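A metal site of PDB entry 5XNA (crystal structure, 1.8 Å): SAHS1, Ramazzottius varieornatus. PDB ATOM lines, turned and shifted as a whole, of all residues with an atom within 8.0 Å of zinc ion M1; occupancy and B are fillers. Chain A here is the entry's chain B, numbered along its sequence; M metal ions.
Within 4 Å of zinc ion M1: His 51, His 53 and Asn 68.
A ring nitrogen (NE2) of His 53 binds zinc ion M1, 2.0 Å away.
NE2 of His 51 is bound to zinc ion M1 (2.1 Å).
OD1 of Asn 68 is bound to zinc ion M1, at 2.3 Å.
Zinc ion M1 has three donor atoms within binding distance.
O of Trp 46 sits at hydrogen-bond distance from N of His 53 (2.9 Å).
A ring nitrogen (ND1) of His 51 sits at hydrogen-bond distance from the backbone carbonyl oxygen of Glu 48, at 2.8 Å.
OD1 of Asp 50 lies within hydrogen-bond range of ND1 of His 51, at 3.1 Å.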
ATOM      1  N   TRP A  46     -18.567 -13.114   0.685  1.00  0.00           N
ATOM      2  CA  TRP A  46     -17.738 -12.722   1.817  1.00  0.00           C
ATOM      3  C   TRP A  46     -18.326 -13.313   3.092  1.00  0.00           C
ATOM      4  O   TRP A  46     -19.430 -13.869   3.090  1.00  0.00           O
ATOM      5  CB  TRP A  46     -17.584 -11.197   1.889  1.00  0.00           C
ATOM      6  CG  TRP A  46     -18.823 -10.428   2.293  1.00  0.00           C
ATOM      7  CD1 TRP A  46     -19.099  -9.954   3.542  1.00  0.00           C
ATOM      8  CD2 TRP A  46     -19.916 -10.026   1.448  1.00  0.00           C
ATOM      9  NE1 TRP A  46     -20.298  -9.282   3.529  1.00  0.00           N
ATOM     10  CE2 TRP A  46     -20.818  -9.304   2.258  1.00  0.00           C
ATOM     11  CE3 TRP A  46     -20.214 -10.196   0.087  1.00  0.00           C
ATOM     12  CZ2 TRP A  46     -22.003  -8.757   1.756  1.00  0.00           C
ATOM     13  CZ3 TRP A  46     -21.400  -9.662  -0.397  1.00  0.00           C
ATOM     14  CH2 TRP A  46     -22.277  -8.966   0.435  1.00  0.00           C
ATOM     15  N   LYS A  47     -17.578 -13.215   4.183  1.00  0.00           N
ATOM     16  CA  LYS A  47     -17.969 -13.809   5.446  1.00  0.00           C
ATOM     17  C   LYS A  47     -18.445 -12.735   6.427  1.00  0.00           C
ATOM     18  O   LYS A  47     -17.905 -11.617   6.454  1.00  0.00           O
ATOM     19  CB  LYS A  47     -16.810 -14.595   6.065  1.00  0.00           C
ATOM     20  CG  LYS A  47     -17.203 -15.399   7.278  1.00  0.00           C
ATOM     21  CD  LYS A  47     -16.052 -16.293   7.736  1.00  0.00           C
ATOM     22  CE  LYS A  47     -16.590 -17.465   8.558  1.00  0.00           C
ATOM     23  NZ  LYS A  47     -15.490 -18.302   9.100  1.00  0.00           N
ATOM     24  N   GLU A  48     -19.478 -13.065   7.201  1.00  0.00           N
ATOM     25  CA  GLU A  48     -19.999 -12.224   8.284  1.00  0.00           C
ATOM     26  C   GLU A  48     -20.181 -13.115   9.501  1.00  0.00           C
ATOM     27  O   GLU A  48     -21.166 -13.854   9.599  1.00  0.00           O
ATOM     28  CB  GLU A  48     -21.328 -11.569   7.908  1.00  0.00           C
ATOM     29  CG  GLU A  48     -21.285 -10.595   6.761  1.00  0.00           C
ATOM     30  CD  GLU A  48     -20.587  -9.311   7.114  1.00  0.00           C
ATOM     31  OE1 GLU A  48     -20.156  -9.160   8.274  1.00  0.00           O
ATOM     32  OE2 GLU A  48     -20.457  -8.450   6.229  1.00  0.00           O
ATOM     33  N   GLY A  49     -19.222 -13.063  10.426  1.00  0.00           N
ATOM     34  CA  GLY A  49     -19.325 -13.833  11.638  1.00  0.00           C
ATOM     35  C   GLY A  49     -19.409 -15.308  11.334  1.00  0.00           C
ATOM     36  O   GLY A  49     -18.467 -15.897  10.793  1.00  0.00           O
ATOM     37  N   ASP A  50     -20.551 -15.900  11.649  1.00  0.00           N
ATOM     38  CA  ASP A  50     -20.768 -17.333  11.552  1.00  0.00           C
ATOM     39  C   ASP A  50     -21.341 -17.769  10.214  1.00  0.00           C
ATOM     40  O   ASP A  50     -21.603 -18.969  10.037  1.00  0.00           O
ATOM     41  CB  ASP A  50     -21.668 -17.802  12.719  1.00  0.00           C
ATOM     42  CG  ASP A  50     -23.012 -17.031  12.810  1.00  0.00           C
ATOM     43  OD1 ASP A  50     -23.242 -15.985  12.145  1.00  0.00           O
ATOM     44  OD2 ASP A  50     -23.870 -17.487  13.603  1.00  0.00           O
ATOM     45  N   HIS A  51     -21.538 -16.856   9.267  1.00  0.00           N
ATOM     46  CA  HIS A  51     -22.228 -17.170   8.025  1.00  0.00           C
ATOM     47  C   HIS A  51     -21.583 -16.411   6.879  1.00  0.00           C
ATOM     48  O   HIS A  51     -20.608 -15.666   7.048  1.00  0.00           O
ATOM     49  CB  HIS A  51     -23.731 -16.848   8.122  1.00  0.00           C
ATOM     50  CG  HIS A  51     -24.033 -15.381   8.265  1.00  0.00           C
ATOM     51  ND1 HIS A  51     -23.850 -14.683   9.449  1.00  0.00           N
ATOM     52  CD2 HIS A  51     -24.524 -14.485   7.382  1.00  0.00           C
ATOM     53  CE1 HIS A  51     -24.220 -13.425   9.281  1.00  0.00           C
ATOM     54  NE2 HIS A  51     -24.640 -13.274   8.030  1.00  0.00           N
ATOM     55  N   TYR A  52     -22.158 -16.598   5.677  1.00  0.00           N
ATOM     56  CA  TYR A  52     -21.622 -15.994   4.475  1.00  0.00           C
ATOM     57  C   TYR A  52     -22.716 -15.200   3.766  1.00  0.00           C
ATOM     58  O   TYR A  52     -23.917 -15.443   3.941  1.00  0.00           O
ATOM     59  CB  TYR A  52     -21.065 -17.034   3.482  1.00  0.00           C
ATOM     60  CG  TYR A  52     -19.834 -17.763   3.962  1.00  0.00           C
ATOM     61  CD1 TYR A  52     -19.940 -18.897   4.751  1.00  0.00           C
ATOM     62  CD2 TYR A  52     -18.575 -17.326   3.596  1.00  0.00           C
ATOM     63  CE1 TYR A  52     -18.813 -19.574   5.192  1.00  0.00           C
ATOM     64  CE2 TYR A  52     -17.430 -18.002   4.027  1.00  0.00           C
ATOM     65  CZ  TYR A  52     -17.568 -19.117   4.822  1.00  0.00           C
ATOM     66  OH  TYR A  52     -16.459 -19.790   5.248  1.00  0.00           O
ATOM     67  N   HIS A  53     -22.269 -14.257   2.958  1.00  0.00           N
ATOM     68  CA  HIS A  53     -23.124 -13.486   2.074  1.00  0.00           C
ATOM     69  C   HIS A  53     -22.720 -13.781   0.638  1.00  0.00           C
ATOM     70  O   HIS A  53     -21.533 -13.895   0.324  1.00  0.00           O
ATOM     71  CB  HIS A  53     -23.007 -11.989   2.335  1.00  0.00           C
ATOM     72  CG  HIS A  53     -23.661 -11.541   3.613  1.00  0.00           C
ATOM     73  ND1 HIS A  53     -23.905 -10.226   3.893  1.00  0.00           N
ATOM     74  CD2 HIS A  53     -24.089 -12.249   4.682  1.00  0.00           C
ATOM     75  CE1 HIS A  53     -24.486 -10.131   5.072  1.00  0.00           C
ATOM     76  NE2 HIS A  53     -24.610 -11.353   5.576  1.00  0.00           N
ATOM     77  N   ASP A  66     -29.286 -10.745  -2.794  1.00  0.00           N
ATOM     78  CA  ASP A  66     -28.346 -10.928  -1.694  1.00  0.00           C
ATOM     79  C   ASP A  66     -28.764 -12.162  -0.911  1.00  0.00           C
ATOM     80  O   ASP A  66     -29.895 -12.217  -0.401  1.00  0.00           O
ATOM     81  CB  ASP A  66     -28.288  -9.708  -0.776  1.00  0.00           C
ATOM     82  CG  ASP A  66     -26.951  -9.577  -0.069  1.00  0.00           C
ATOM     83  OD1 ASP A  66     -26.652 -10.435   0.796  1.00  0.00           O
ATOM     84  OD2 ASP A  66     -26.199  -8.628  -0.372  1.00  0.00           O
ATOM     85  N   VAL A  67     -27.874 -13.143  -0.837  1.00  0.00           N
ATOM     86  CA  VAL A  67     -28.157 -14.430  -0.214  1.00  0.00           C
ATOM     87  C   VAL A  67     -27.322 -14.542   1.061  1.00  0.00           C
ATOM     88  O   VAL A  67     -26.112 -14.334   1.029  1.00  0.00           O
ATOM     89  CB  VAL A  67     -27.824 -15.589  -1.176  1.00  0.00           C
ATOM     90  CG1 VAL A  67     -28.108 -16.916  -0.516  1.00  0.00           C
ATOM     91  CG2 VAL A  67     -28.629 -15.454  -2.477  1.00  0.00           C
ATOM     92  N   ASN A  68     -27.969 -14.892   2.167  1.00  0.00           N
ATOM     93  CA  ASN A  68     -27.294 -15.262   3.406  1.00  0.00           C
ATOM     94  C   ASN A  68     -27.231 -16.782   3.469  1.00  0.00           C
ATOM     95  O   ASN A  68     -28.263 -17.447   3.289  1.00  0.00           O
ATOM     96  CB  ASN A  68     -28.049 -14.726   4.630  1.00  0.00           C
ATOM     97  CG  ASN A  68     -27.604 -13.333   5.053  1.00  0.00           C
ATOM     98  OD1 ASN A  68     -26.767 -13.195   5.951  1.00  0.00           O
ATOM     99  ND2 ASN A  68     -28.182 -12.301   4.456  1.00  0.00           N
ATOM    100  N   PHE A  69     -26.063 -17.343   3.742  1.00  0.00           N
ATOM    101  CA  PHE A  69     -26.011 -18.793   3.924  1.00  0.00           C
ATOM    102  C   PHE A  69     -25.024 -19.193   4.999  1.00  0.00           C
ATOM    103  O   PHE A  69     -23.978 -18.562   5.183  1.00  0.00           O
ATOM    104  CB  PHE A  69     -25.693 -19.531   2.592  1.00  0.00           C
ATOM    105  CG  PHE A  69     -24.264 -19.392   2.081  1.00  0.00           C
ATOM    106  CD1 PHE A  69     -23.271 -20.267   2.498  1.00  0.00           C
ATOM    107  CD2 PHE A  69     -23.942 -18.476   1.092  1.00  0.00           C
ATOM    108  CE1 PHE A  69     -21.987 -20.192   1.980  1.00  0.00           C
ATOM    109  CE2 PHE A  69     -22.668 -18.409   0.555  1.00  0.00           C
ATOM    110  CZ  PHE A  69     -21.685 -19.263   1.000  1.00  0.00           C
HETATM  111 ZN    ZN M   1     -25.663 -11.666   7.252  1.00  0.00          ZN
HETATM  112 ZN    ZN M   2     -19.224  -7.438   9.093  1.00  0.00          ZN
